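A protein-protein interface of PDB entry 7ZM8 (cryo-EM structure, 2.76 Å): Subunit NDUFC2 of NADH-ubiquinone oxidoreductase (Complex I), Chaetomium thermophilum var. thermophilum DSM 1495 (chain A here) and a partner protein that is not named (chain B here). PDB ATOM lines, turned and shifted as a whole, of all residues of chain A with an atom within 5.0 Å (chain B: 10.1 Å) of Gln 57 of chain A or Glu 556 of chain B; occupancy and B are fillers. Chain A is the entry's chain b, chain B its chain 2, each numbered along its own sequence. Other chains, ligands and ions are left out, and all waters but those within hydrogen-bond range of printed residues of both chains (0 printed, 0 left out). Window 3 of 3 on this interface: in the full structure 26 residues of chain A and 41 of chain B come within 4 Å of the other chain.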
ATOM      1  N   ARG A   4     -17.284  17.407 -22.050  1.00  0.00           N
ATOM      2  CA  ARG A   4     -17.559  18.532 -21.125  1.00  0.00           C
ATOM      3  C   ARG A   4     -16.330  19.426 -21.092  1.00  0.00           C
ATOM      4  O   ARG A   4     -16.490  20.645 -21.022  1.00  0.00           O
ATOM      5  CB  ARG A   4     -17.761  18.010 -19.701  1.00  0.00           C
ATOM      6  CG  ARG A   4     -19.187  18.123 -19.188  1.00  0.00           C
ATOM      7  CD  ARG A   4     -19.270  17.690 -17.738  1.00  0.00           C
ATOM      8  NE  ARG A   4     -18.685  16.376 -17.522  1.00  0.00           N
ATOM      9  CZ  ARG A   4     -19.358  15.231 -17.574  1.00  0.00           C
ATOM     10  NH1 ARG A   4     -18.735  14.087 -17.358  1.00  0.00           N
ATOM     11  NH2 ARG A   4     -20.651  15.234 -17.843  1.00  0.00           N
ATOM     12  N   LEU A  50     -17.216  19.523 -12.931  1.00  0.00           N
ATOM     13  CA  LEU A  50     -18.525  18.966 -13.355  1.00  0.00           C
ATOM     14  C   LEU A  50     -18.386  17.485 -13.689  1.00  0.00           C
ATOM     15  O   LEU A  50     -19.396  16.793 -13.669  1.00  0.00           O
ATOM     16  CB  LEU A  50     -19.105  19.783 -14.514  1.00  0.00           C
ATOM     17  CG  LEU A  50     -19.760  21.099 -14.104  1.00  0.00           C
ATOM     18  CD1 LEU A  50     -20.674  21.601 -15.203  1.00  0.00           C
ATOM     19  CD2 LEU A  50     -20.545  20.923 -12.816  1.00  0.00           C
ATOM     20  N   ILE A  53     -18.628  15.968 -10.355  1.00  0.00           N
ATOM     21  CA  ILE A  53     -20.030  16.059  -9.963  1.00  0.00           C
ATOM     22  C   ILE A  53     -20.846  14.992 -10.677  1.00  0.00           C
ATOM     23  O   ILE A  53     -21.674  14.305 -10.070  1.00  0.00           O
ATOM     24  CB  ILE A  53     -20.573  17.470 -10.248  1.00  0.00           C
ATOM     25  CG1 ILE A  53     -19.827  18.506  -9.414  1.00  0.00           C
ATOM     26  CG2 ILE A  53     -22.059  17.544  -9.969  1.00  0.00           C
ATOM     27  CD1 ILE A  53     -20.073  18.383  -7.938  1.00  0.00           C
ATOM     28  N   ASP A  54     -20.624  14.838 -11.980  1.00  0.00           N
ATOM     29  CA  ASP A  54     -21.393  13.865 -12.742  1.00  0.00           C
ATOM     30  C   ASP A  54     -21.094  12.445 -12.293  1.00  0.00           C
ATOM     31  O   ASP A  54     -21.995  11.603 -12.229  1.00  0.00           O
ATOM     32  CB  ASP A  54     -21.112  14.017 -14.232  1.00  0.00           C
ATOM     33  CG  ASP A  54     -22.009  13.148 -15.072  1.00  0.00           C
ATOM     34  OD1 ASP A  54     -23.233  13.171 -14.832  1.00  0.00           O
ATOM     35  OD2 ASP A  54     -21.501  12.433 -15.960  1.00  0.00           O
ATOM     36  N   GLU A  55     -19.827  12.157 -11.991  1.00  0.00           N
ATOM     37  CA  GLU A  55     -19.451  10.814 -11.572  1.00  0.00           C
ATOM     38  C   GLU A  55     -20.197  10.414 -10.310  1.00  0.00           C
ATOM     39  O   GLU A  55     -20.681   9.282 -10.199  1.00  0.00           O
ATOM     40  CB  GLU A  55     -17.940  10.749 -11.349  1.00  0.00           C
ATOM     41  CG  GLU A  55     -17.400   9.387 -10.951  1.00  0.00           C
ATOM     42  CD  GLU A  55     -17.566   8.343 -12.040  1.00  0.00           C
ATOM     43  OE1 GLU A  55     -17.631   8.723 -13.228  1.00  0.00           O
ATOM     44  OE2 GLU A  55     -17.621   7.140 -11.708  1.00  0.00           O
ATOM     45  N   LYS A  56     -20.307  11.334  -9.351  1.00  0.00           N
ATOM     46  CA  LYS A  56     -20.968  11.035  -8.090  1.00  0.00           C
ATOM     47  C   LYS A  56     -22.484  11.026  -8.231  1.00  0.00           C
ATOM     48  O   LYS A  56     -23.160  10.208  -7.600  1.00  0.00           O
ATOM     49  CB  LYS A  56     -20.533  12.042  -7.031  1.00  0.00           C
ATOM     50  CG  LYS A  56     -19.029  12.061  -6.737  1.00  0.00           C
ATOM     51  CD  LYS A  56     -18.537  10.818  -5.994  1.00  0.00           C
ATOM     52  CE  LYS A  56     -18.011   9.741  -6.940  1.00  0.00           C
ATOM     53  NZ  LYS A  56     -17.437   8.584  -6.199  1.00  0.00           N
ATOM     54  N   GLN A  57     -23.036  11.922  -9.050  1.00  0.00           N
ATOM     55  CA  GLN A  57     -24.472  11.914  -9.302  1.00  0.00           C
ATOM     56  C   GLN A  57     -24.906  10.613  -9.954  1.00  0.00           C
ATOM     57  O   GLN A  57     -25.990  10.096  -9.664  1.00  0.00           O
ATOM     58  CB  GLN A  57     -24.860  13.090 -10.192  1.00  0.00           C
ATOM     59  CG  GLN A  57     -24.923  14.421  -9.494  1.00  0.00           C
ATOM     60  CD  GLN A  57     -25.020  15.561 -10.469  1.00  0.00           C
ATOM     61  OE1 GLN A  57     -24.761  15.393 -11.657  1.00  0.00           O
ATOM     62  NE2 GLN A  57     -25.396  16.726  -9.980  1.00  0.00           N
ATOM     63  N   THR A  58     -24.084  10.086 -10.859  1.00  0.00           N
ATOM     64  CA  THR A  58     -24.401   8.823 -11.512  1.00  0.00           C
ATOM     65  C   THR A  58     -24.476   7.689 -10.502  1.00  0.00           C
ATOM     66  O   THR A  58     -25.371   6.842 -10.572  1.00  0.00           O
ATOM     67  CB  THR A  58     -23.362   8.520 -12.587  1.00  0.00           C
ATOM     68  OG1 THR A  58     -23.343   9.584 -13.544  1.00  0.00           O
ATOM     69  CG2 THR A  58     -23.686   7.216 -13.292  1.00  0.00           C
ATOM     70  N   LYS A  59     -23.543   7.657  -9.553  1.00  0.00           N
ATOM     71  CA  LYS A  59     -23.546   6.602  -8.551  1.00  0.00           C
ATOM     72  C   LYS A  59     -24.798   6.661  -7.692  1.00  0.00           C
ATOM     73  O   LYS A  59     -25.379   5.625  -7.352  1.00  0.00           O
ATOM     74  CB  LYS A  59     -22.297   6.707  -7.680  1.00  0.00           C
ATOM     75  CG  LYS A  59     -21.001   6.548  -8.440  1.00  0.00           C
ATOM     76  CD  LYS A  59     -20.905   5.181  -9.086  1.00  0.00           C
ATOM     77  CE  LYS A  59     -20.797   4.088  -8.038  1.00  0.00           C
ATOM     78  NZ  LYS A  59     -19.535   4.200  -7.257  1.00  0.00           N
ATOM     79  N   MET A  60     -25.222   7.863  -7.317  1.00  0.00           N
ATOM     80  CA  MET A  60     -26.334   7.985  -6.387  1.00  0.00           C
ATOM     81  C   MET A  60     -27.679   7.850  -7.089  1.00  0.00           C
ATOM     82  O   MET A  60     -28.635   7.336  -6.501  1.00  0.00           O
ATOM     83  CB  MET A  60     -26.232   9.304  -5.626  1.00  0.00           C
ATOM     84  CG  MET A  60     -27.023   9.294  -4.335  1.00  0.00           C
ATOM     85  SD  MET A  60     -27.564  10.918  -3.816  1.00  0.00           S
ATOM     86  CE  MET A  60     -26.002  11.540  -3.212  1.00  0.00           C
ATOM     87  N   LEU A  61     -27.785   8.304  -8.335  1.00  0.00           N
ATOM     88  CA  LEU A  61     -29.013   8.052  -9.075  1.00  0.00           C
ATOM     89  C   LEU A  61     -29.153   6.581  -9.429  1.00  0.00           C
ATOM     90  O   LEU A  61     -30.275   6.075  -9.521  1.00  0.00           O
ATOM     91  CB  LEU A  61     -29.068   8.912 -10.336  1.00  0.00           C
ATOM     92  CG  LEU A  61     -29.499  10.361 -10.122  1.00  0.00           C
ATOM     93  CD1 LEU A  61     -29.333  11.161 -11.391  1.00  0.00           C
ATOM     94  CD2 LEU A  61     -30.928  10.423  -9.626  1.00  0.00           C
ATOM     95  N   GLU A  62     -28.038   5.884  -9.642  1.00  0.00           N
ATOM     96  CA  GLU A  62     -28.096   4.443  -9.851  1.00  0.00           C
ATOM     97  C   GLU A  62     -28.584   3.725  -8.602  1.00  0.00           C
ATOM     98  O   GLU A  62     -29.420   2.818  -8.685  1.00  0.00           O
ATOM     99  CB  GLU A  62     -26.725   3.914 -10.263  1.00  0.00           C
ATOM    100  CG  GLU A  62     -26.464   3.977 -11.754  1.00  0.00           C
ATOM    101  CD  GLU A  62     -27.374   3.060 -12.545  1.00  0.00           C
ATOM    102  OE1 GLU A  62     -27.600   1.917 -12.097  1.00  0.00           O
ATOM    103  OE2 GLU A  62     -27.865   3.482 -13.613  1.00  0.00           O
ATOM    104  N   LEU B  44     -22.290  19.422   2.670  1.00  0.00           N
ATOM    105  CA  LEU B  44     -23.021  18.530   1.780  1.00  0.00           C
ATOM    106  C   LEU B  44     -22.252  17.215   1.717  1.00  0.00           C
ATOM    107  O   LEU B  44     -21.481  16.967   0.791  1.00  0.00           O
ATOM    108  CB  LEU B  44     -23.151  19.171   0.395  1.00  0.00           C
ATOM    109  CG  LEU B  44     -24.002  20.421   0.217  1.00  0.00           C
ATOM    110  CD1 LEU B  44     -23.728  21.018  -1.131  1.00  0.00           C
ATOM    111  CD2 LEU B  44     -25.453  20.047   0.314  1.00  0.00           C
ATOM    112  N   ILE B  47     -26.969  12.160   3.301  1.00  0.00           N
ATOM    113  CA  ILE B  47     -28.284  12.027   2.626  1.00  0.00           C
ATOM    114  C   ILE B  47     -29.309  12.014   3.752  1.00  0.00           C
ATOM    115  O   ILE B  47     -29.327  11.060   4.526  1.00  0.00           O
ATOM    116  CB  ILE B  47     -28.349  10.747   1.784  1.00  0.00           C
ATOM    117  CG1 ILE B  47     -27.446  10.849   0.559  1.00  0.00           C
ATOM    118  CG2 ILE B  47     -29.782  10.442   1.384  1.00  0.00           C
ATOM    119  CD1 ILE B  47     -27.663  12.114  -0.222  1.00  0.00           C
ATOM    120  N   ILE B  66     -27.992  23.438  -0.378  1.00  0.00           N
ATOM    121  CA  ILE B  66     -27.849  23.790  -1.786  1.00  0.00           C
ATOM    122  C   ILE B  66     -28.312  25.221  -2.026  1.00  0.00           C
ATOM    123  O   ILE B  66     -27.657  25.987  -2.738  1.00  0.00           O
ATOM    124  CB  ILE B  66     -28.610  22.779  -2.669  1.00  0.00           C
ATOM    125  CG1 ILE B  66     -27.805  21.486  -2.826  1.00  0.00           C
ATOM    126  CG2 ILE B  66     -28.928  23.368  -4.027  1.00  0.00           C
ATOM    127  CD1 ILE B  66     -26.659  21.579  -3.802  1.00  0.00           C
ATOM    128  N   ILE B 367     -37.700  23.498  -8.756  1.00  0.00           N
ATOM    129  CA  ILE B 367     -36.299  23.839  -8.380  1.00  0.00           C
ATOM    130  C   ILE B 367     -35.621  24.488  -9.586  1.00  0.00           C
ATOM    131  O   ILE B 367     -34.946  25.516  -9.414  1.00  0.00           O
ATOM    132  CB  ILE B 367     -35.527  22.615  -7.845  1.00  0.00           C
ATOM    133  CG1 ILE B 367     -36.202  22.016  -6.611  1.00  0.00           C
ATOM    134  CG2 ILE B 367     -34.072  22.953  -7.566  1.00  0.00           C
ATOM    135  CD1 ILE B 367     -36.421  23.006  -5.495  1.00  0.00           C
ATOM    136  N   PHE B 368     -35.833  23.928 -10.774  1.00  0.00           N
ATOM    137  CA  PHE B 368     -35.245  24.523 -11.995  1.00  0.00           C
ATOM    138  C   PHE B 368     -35.838  25.898 -12.299  1.00  0.00           C
ATOM    139  O   PHE B 368     -35.050  26.804 -12.575  1.00  0.00           O
ATOM    140  CB  PHE B 368     -35.391  23.570 -13.175  1.00  0.00           C
ATOM    141  CG  PHE B 368     -34.694  24.055 -14.419  1.00  0.00           C
ATOM    142  CD1 PHE B 368     -33.327  24.264 -14.423  1.00  0.00           C
ATOM    143  CD2 PHE B 368     -35.404  24.311 -15.579  1.00  0.00           C
ATOM    144  CE1 PHE B 368     -32.686  24.724 -15.560  1.00  0.00           C
ATOM    145  CE2 PHE B 368     -34.759  24.765 -16.715  1.00  0.00           C
ATOM    146  CZ  PHE B 368     -33.405  24.977 -16.703  1.00  0.00           C
ATOM    147  N   ILE B 371     -34.323  28.581  -9.862  1.00  0.00           N
ATOM    148  CA  ILE B 371     -32.917  28.931 -10.039  1.00  0.00           C
ATOM    149  C   ILE B 371     -32.693  29.619 -11.378  1.00  0.00           C
ATOM    150  O   ILE B 371     -32.049  30.669 -11.449  1.00  0.00           O
ATOM    151  CB  ILE B 371     -32.020  27.690  -9.892  1.00  0.00           C
ATOM    152  CG1 ILE B 371     -31.836  27.331  -8.422  1.00  0.00           C
ATOM    153  CG2 ILE B 371     -30.658  27.942 -10.498  1.00  0.00           C
ATOM    154  CD1 ILE B 371     -31.062  26.061  -8.209  1.00  0.00           C
ATOM    155  N   LEU B 549     -26.557  28.371 -24.307  1.00  0.00           N
ATOM    156  CA  LEU B 549     -25.910  27.082 -24.487  1.00  0.00           C
ATOM    157  C   LEU B 549     -26.393  26.034 -23.500  1.00  0.00           C
ATOM    158  O   LEU B 549     -25.708  25.030 -23.301  1.00  0.00           O
ATOM    159  CB  LEU B 549     -24.394  27.240 -24.375  1.00  0.00           C
ATOM    160  CG  LEU B 549     -23.726  28.272 -25.283  1.00  0.00           C
ATOM    161  CD1 LEU B 549     -22.276  28.432 -24.906  1.00  0.00           C
ATOM    162  CD2 LEU B 549     -23.856  27.878 -26.731  1.00  0.00           C
ATOM    163  N   PHE B 550     -27.567  26.232 -22.900  1.00  0.00           N
ATOM    164  CA  PHE B 550     -28.046  25.321 -21.864  1.00  0.00           C
ATOM    165  C   PHE B 550     -28.234  23.905 -22.387  1.00  0.00           C
ATOM    166  O   PHE B 550     -28.033  22.941 -21.643  1.00  0.00           O
ATOM    167  CB  PHE B 550     -29.357  25.852 -21.277  1.00  0.00           C
ATOM    168  CG  PHE B 550     -30.066  24.882 -20.373  1.00  0.00           C
ATOM    169  CD1 PHE B 550     -29.706  24.759 -19.043  1.00  0.00           C
ATOM    170  CD2 PHE B 550     -31.102  24.098 -20.852  1.00  0.00           C
ATOM    171  CE1 PHE B 550     -30.358  23.872 -18.214  1.00  0.00           C
ATOM    172  CE2 PHE B 550     -31.752  23.208 -20.028  1.00  0.00           C
ATOM    173  CZ  PHE B 550     -31.385  23.100 -18.709  1.00  0.00           C
ATOM    174  N   ILE B 551     -28.595  23.758 -23.664  1.00  0.00           N
ATOM    175  CA  ILE B 551     -28.938  22.424 -24.231  1.00  0.00           C
ATOM    176  C   ILE B 551     -27.682  21.587 -24.450  1.00  0.00           C
ATOM    177  O   ILE B 551     -27.800  20.474 -24.974  1.00  0.00           O
ATOM    178  CB  ILE B 551     -29.755  22.628 -25.514  1.00  0.00           C
ATOM    179  CG1 ILE B 551     -30.657  21.430 -25.825  1.00  0.00           C
ATOM    180  CG2 ILE B 551     -28.876  23.009 -26.690  1.00  0.00           C
ATOM    181  CD1 ILE B 551     -31.529  21.618 -27.039  1.00  0.00           C
ATOM    182  N   PHE B 552     -26.522  22.112 -24.078  1.00  0.00           N
ATOM    183  CA  PHE B 552     -25.245  21.384 -24.221  1.00  0.00           C
ATOM    184  C   PHE B 552     -24.643  21.188 -22.831  1.00  0.00           C
ATOM    185  O   PHE B 552     -23.608  20.518 -22.718  1.00  0.00           O
ATOM    186  CB  PHE B 552     -24.333  22.170 -25.162  1.00  0.00           C
ATOM    187  CG  PHE B 552     -24.931  22.507 -26.501  1.00  0.00           C
ATOM    188  CD1 PHE B 552     -25.184  21.517 -27.435  1.00  0.00           C
ATOM    189  CD2 PHE B 552     -25.236  23.815 -26.831  1.00  0.00           C
ATOM    190  CE1 PHE B 552     -25.738  21.825 -28.665  1.00  0.00           C
ATOM    191  CE2 PHE B 552     -25.786  24.125 -28.063  1.00  0.00           C
ATOM    192  CZ  PHE B 552     -26.036  23.128 -28.978  1.00  0.00           C
ATOM    193  N   MET B 553     -25.266  21.763 -21.804  1.00  0.00           N
ATOM    194  CA  MET B 553     -24.683  21.741 -20.442  1.00  0.00           C
ATOM    195  C   MET B 553     -25.784  21.493 -19.428  1.00  0.00           C
ATOM    196  O   MET B 553     -25.763  22.142 -18.378  1.00  0.00           O
ATOM    197  CB  MET B 553     -24.070  23.107 -20.130  1.00  0.00           C
ATOM    198  CG  MET B 553     -24.959  24.271 -20.477  1.00  0.00           C
ATOM    199  SD  MET B 553     -24.469  25.845 -19.749  1.00  0.00           S
ATOM    200  CE  MET B 553     -25.094  25.634 -18.084  1.00  0.00           C
ATOM    201  N   ASN B 554     -26.701  20.580 -19.715  1.00  0.00           N
ATOM    202  CA  ASN B 554     -27.888  20.439 -18.832  1.00  0.00           C
ATOM    203  C   ASN B 554     -27.791  19.275 -17.836  1.00  0.00           C
ATOM    204  O   ASN B 554     -28.567  19.302 -16.881  1.00  0.00           O
ATOM    205  CB  ASN B 554     -29.163  20.404 -19.685  1.00  0.00           C
ATOM    206  CG  ASN B 554     -29.199  19.279 -20.695  1.00  0.00           C
ATOM    207  OD1 ASN B 554     -29.630  18.175 -20.384  1.00  0.00           O
ATOM    208  ND2 ASN B 554     -28.767  19.552 -21.914  1.00  0.00           N
ATOM    209  N   LYS B 555     -26.863  18.336 -18.003  1.00  0.00           N
ATOM    210  CA  LYS B 555     -26.877  17.112 -17.146  1.00  0.00           C
ATOM    211  C   LYS B 555     -26.748  17.359 -15.638  1.00  0.00           C
ATOM    212  O   LYS B 555     -27.611  16.865 -14.924  1.00  0.00           O
ATOM    213  CB  LYS B 555     -25.842  16.079 -17.595  1.00  0.00           C
ATOM    214  CG  LYS B 555     -26.142  14.645 -17.182  1.00  0.00           C
ATOM    215  CD  LYS B 555     -25.080  13.664 -17.619  1.00  0.00           C
ATOM    216  CE  LYS B 555     -25.467  12.223 -17.366  1.00  0.00           C
ATOM    217  NZ  LYS B 555     -25.850  11.997 -15.953  1.00  0.00           N
ATOM    218  N   GLU B 556     -25.778  18.140 -15.169  1.00  0.00           N
ATOM    219  CA  GLU B 556     -25.510  18.210 -13.712  1.00  0.00           C
ATOM    220  C   GLU B 556     -26.469  19.170 -13.008  1.00  0.00           C
ATOM    221  O   GLU B 556     -26.727  18.951 -11.825  1.00  0.00           O
ATOM    222  CB  GLU B 556     -24.027  18.509 -13.493  1.00  0.00           C
ATOM    223  CG  GLU B 556     -23.098  17.430 -14.009  1.00  0.00           C
ATOM    224  CD  GLU B 556     -22.791  17.521 -15.492  1.00  0.00           C
ATOM    225  OE1 GLU B 556     -22.235  16.562 -16.041  1.00  0.00           O
ATOM    226  OE2 GLU B 556     -23.115  18.556 -16.091  1.00  0.00           O
ATOM    227  N   TRP B 557     -26.964  20.185 -13.704  1.00  0.00           N
ATOM    228  CA  TRP B 557     -27.974  21.122 -13.154  1.00  0.00           C
ATOM    229  C   TRP B 557     -29.289  20.373 -12.904  1.00  0.00           C
ATOM    230  O   TRP B 557     -29.869  20.537 -11.813  1.00  0.00           O
ATOM    231  CB  TRP B 557     -28.117  22.313 -14.117  1.00  0.00           C
ATOM    232  CG  TRP B 557     -28.921  23.502 -13.684  1.00  0.00           C
ATOM    233  CD1 TRP B 557     -29.716  23.621 -12.585  1.00  0.00           C
ATOM    234  CD2 TRP B 557     -29.014  24.760 -14.375  1.00  0.00           C
ATOM    235  NE1 TRP B 557     -30.295  24.860 -12.545  1.00  0.00           N
ATOM    236  CE2 TRP B 557     -29.880  25.583 -13.628  1.00  0.00           C
ATOM    237  CE3 TRP B 557     -28.452  25.276 -15.547  1.00  0.00           C
ATOM    238  CZ2 TRP B 557     -30.192  26.884 -14.015  1.00  0.00           C
ATOM    239  CZ3 TRP B 557     -28.757  26.563 -15.929  1.00  0.00           C
ATOM    240  CH2 TRP B 557     -29.621  27.353 -15.173  1.00  0.00           C
ATOM    241  N   LEU B 558     -29.744  19.583 -13.872  1.00  0.00           N
ATOM    242  CA  LEU B 558     -31.049  18.896 -13.718  1.00  0.00           C
ATOM    243  C   LEU B 558     -30.891  17.634 -12.872  1.00  0.00           C
ATOM    244  O   LEU B 558     -31.859  17.264 -12.211  1.00  0.00           O
ATOM    245  CB  LEU B 558     -31.625  18.631 -15.109  1.00  0.00           C
ATOM    246  CG  LEU B 558     -32.024  19.872 -15.901  1.00  0.00           C
ATOM    247  CD1 LEU B 558     -32.281  19.522 -17.356  1.00  0.00           C
ATOM    248  CD2 LEU B 558     -33.246  20.531 -15.283  1.00  0.00           C
ATOM    249  N   SER B 559     -29.715  17.012 -12.894  1.00  0.00           N
ATOM    250  CA  SER B 559     -29.412  15.818 -12.058  1.00  0.00           C
ATOM    251  C   SER B 559     -29.440  16.184 -10.576  1.00  0.00           C
ATOM    252  O   SER B 559     -29.838  15.344  -9.779  1.00  0.00           O
ATOM    253  CB  SER B 559     -28.107  15.190 -12.447  1.00  0.00           C
ATOM    254  OG  SER B 559     -28.216  14.488 -13.673  1.00  0.00           O
ATOM    255  N   MET B 560     -28.976  17.380 -10.229  1.00  0.00           N
ATOM    256  CA  MET B 560     -28.972  17.842  -8.828  1.00  0.00           C
ATOM    257  C   MET B 560     -30.405  17.908  -8.331  1.00  0.00           C
ATOM    258  O   MET B 560     -30.660  17.405  -7.241  1.00  0.00           O
ATOM    259  CB  MET B 560     -28.397  19.258  -8.822  1.00  0.00           C
ATOM    260  CG  MET B 560     -28.439  19.952  -7.481  1.00  0.00           C
ATOM    261  SD  MET B 560     -28.259  21.731  -7.710  1.00  0.00           S
ATOM    262  CE  MET B 560     -29.924  22.170  -8.208  1.00  0.00           C
ATOM    263  N   GLY B 561     -31.298  18.492  -9.121  1.00  0.00           N
ATOM    264  CA  GLY B 561     -32.724  18.564  -8.775  1.00  0.00           C
ATOM    265  C   GLY B 561     -33.404  17.214  -8.750  1.00  0.00           C
ATOM    266  O   GLY B 561     -34.260  17.035  -7.887  1.00  0.00           O
ATOM    267  N   THR B 562     -33.065  16.309  -9.667  1.00  0.00           N
ATOM    268  CA  THR B 562     -33.648  14.947  -9.601  1.00  0.00           C
ATOM    269  C   THR B 562     -33.246  14.276  -8.290  1.00  0.00           C
ATOM    270  O   THR B 562     -34.131  13.697  -7.674  1.00  0.00           O
ATOM    271  CB  THR B 562     -33.470  14.109 -10.877  1.00  0.00           C
ATOM    272  OG1 THR B 562     -34.182  12.888 -10.681  1.00  0.00           O
ATOM    273  CG2 THR B 562     -32.041  13.761 -11.210  1.00  0.00           C
ATOM    274  N   ILE B 563     -31.995  14.431  -7.859  1.00  0.00           N
ATOM    275  CA  ILE B 563     -31.521  13.852  -6.569  1.00  0.00           C
ATOM    276  C   ILE B 563     -32.170  14.579  -5.385  1.00  0.00           C
ATOM    277  O   ILE B 563     -32.561  13.887  -4.435  1.00  0.00           O
ATOM    278  CB  ILE B 563     -29.988  13.873  -6.501  1.00  0.00           C
ATOM    279  CG1 ILE B 563     -29.358  13.007  -7.591  1.00  0.00           C
ATOM    280  CG2 ILE B 563     -29.494  13.477  -5.122  1.00  0.00           C
ATOM    281  CD1 ILE B 563     -27.857  13.096  -7.654  1.00  0.00           C
ATOM    282  N   LEU B 564     -32.305  15.905  -5.424  1.00  0.00           N
ATOM    283  CA  LEU B 564     -32.841  16.602  -4.228  1.00  0.00           C
ATOM    284  C   LEU B 564     -34.280  16.155  -3.996  1.00  0.00           C
ATOM    285  O   LEU B 564     -34.630  15.890  -2.836  1.00  0.00           O
ATOM    286  CB  LEU B 564     -32.721  18.126  -4.362  1.00  0.00           C
ATOM    287  CG  LEU B 564     -31.307  18.698  -4.341  1.00  0.00           C
ATOM    288  CD1 LEU B 564     -31.328  20.192  -4.619  1.00  0.00           C
ATOM    289  CD2 LEU B 564     -30.626  18.409  -3.017  1.00  0.00           C
ATOM    290  N   GLN B 566     -35.566  13.358  -4.942  1.00  0.00           N
ATOM    291  CA  GLN B 566     -35.663  11.914  -4.656  1.00  0.00           C
ATOM    292  C   GLN B 566     -35.509  11.750  -3.152  1.00  0.00           C
ATOM    293  O   GLN B 566     -36.200  10.907  -2.633  1.00  0.00           O
ATOM    294  CB  GLN B 566     -34.657  11.078  -5.455  1.00  0.00           C
ATOM    295  CG  GLN B 566     -35.024  10.833  -6.914  1.00  0.00           C
ATOM    296  CD  GLN B 566     -36.367  10.188  -7.159  1.00  0.00           C
ATOM    297  OE1 GLN B 566     -36.675   9.115  -6.655  1.00  0.00           O
ATOM    298  NE2 GLN B 566     -37.173  10.834  -7.979  1.00  0.00           N
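Of the 23 printed residues of chain B, 7 touch a printed residue of chain A.
Of the 12 printed residues of chain A, 6 touch a printed residue of chain B.
Hydrophobic or aromatic side chains of chain A that line the printed part of chain B: Met 60 and Leu 61.
Among the printed residues, Asp or Glu carboxylates within 4 Å of a Lys or Arg side-chain nitrogen of the other chain: Arg 4 of chain A with Glu 556 of chain B (2.7 Å) and Asp 54 of chain A with Lys 555 of chain B (3.1 Å).
Leu 50 of chain A touches Glu 556 of chain B.
Glu 556 of chain B touches Asp 54 of chain A (OE1 to CB, 3.3 Å).
Gln 57 of chain A touches Ser 559 of chain B (OE1 to CB, 3.4 Å).
Met 560 of chain B touches Gln 57 of chain A (N to NE2, 3.6 Å).
Gln 57 of chain A touches Ile 563 of chain B (CG to CD1, 3.7 Å).
Met 60 of chain A touches Ile 47 of chain B (CE to CD1, 3.5 Å).
SD of Met 60 of chain A touches CG2 of Ile 563 of chain B (3.5 Å).
Leu 61 of chain A touches Thr 562 of chain B (CD1 to CG2, 3.8 Å).
Ile 563 of chain B touches Leu 61 of chain A.
The backbone carbonyl oxygen (O) of Lys 555 of chain B is in hydrogen-bond range of the side-chain hydroxyl (OG) of Ser 559 of chain B.
OD2 of Asp 54 of chain A is in salt-bridge range of NH2 of Arg 4 of chain A.
The backbone carbonyl oxygen (O) of Asp 54 of chain A lies within hydrogen-bond range of the side-chain hydroxyl (OG1) of Thr 58 of chain A.
The side-chain amide nitrogen of Gln 57 of chain A lies within hydrogen-bond range of the backbone carbonyl oxygen of Glu 556 of chain B (3.2 Å).
The guanidinium group (NH2) of Arg 4 of chain A is in salt-bridge range of the side-chain carboxylate (OE1) of Glu 556 of chain B (2.7 Å).
The side-chain carboxylate (OD1) of Asp 54 of chain A is in salt-bridge range of the side-chain amino group (NZ) of Lys 555 of chain B, at 3.1 Å.
Gln 57 of chain A touches just these residues of chain B: Glu 556 (3.2 Å), Ser 559 (3.4 Å), Met 560 (3.6 Å) and Ile 563 (3.7 Å).
Glu 556 of chain B touches just these residues of chain A: Arg 4, Leu 50, Asp 54 and Gln 57.
No residue of chain B comes within 4 Å of Ile 53 of chain A.
Of the printed residues of chain B, Asp 54 of chain A touches Lys 555 (3.1 Å) and Glu 556 (3.3 Å).
No residue of chain B comes within 4 Å of Thr 58 of chain A.
Of the printed residues of chain A, Ser 559 of chain B touches Gln 57 (3.4 Å).
Of the printed residues of chain A, Ile 47 of chain B touches Met 60 (3.5 Å).
Of the printed residues of chain B, Met 60 of chain A touches Ile 47 and Ile 563.
Printed residues of chain B within 4 Å of Arg 4 of chain A: Glu 556.
Glu 62 of chain A touches none of the printed residues of chain B.
Leu 564 of chain B touches none of the printed residues of chain A.
The nearest residue of chain B that does not touch Gln 57 of chain A is Lys 555 of chain B (4.6 Å).
The nearest residue of chain A that does not touch Glu 556 of chain B is Ile 53 of chain A (4.2 Å).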
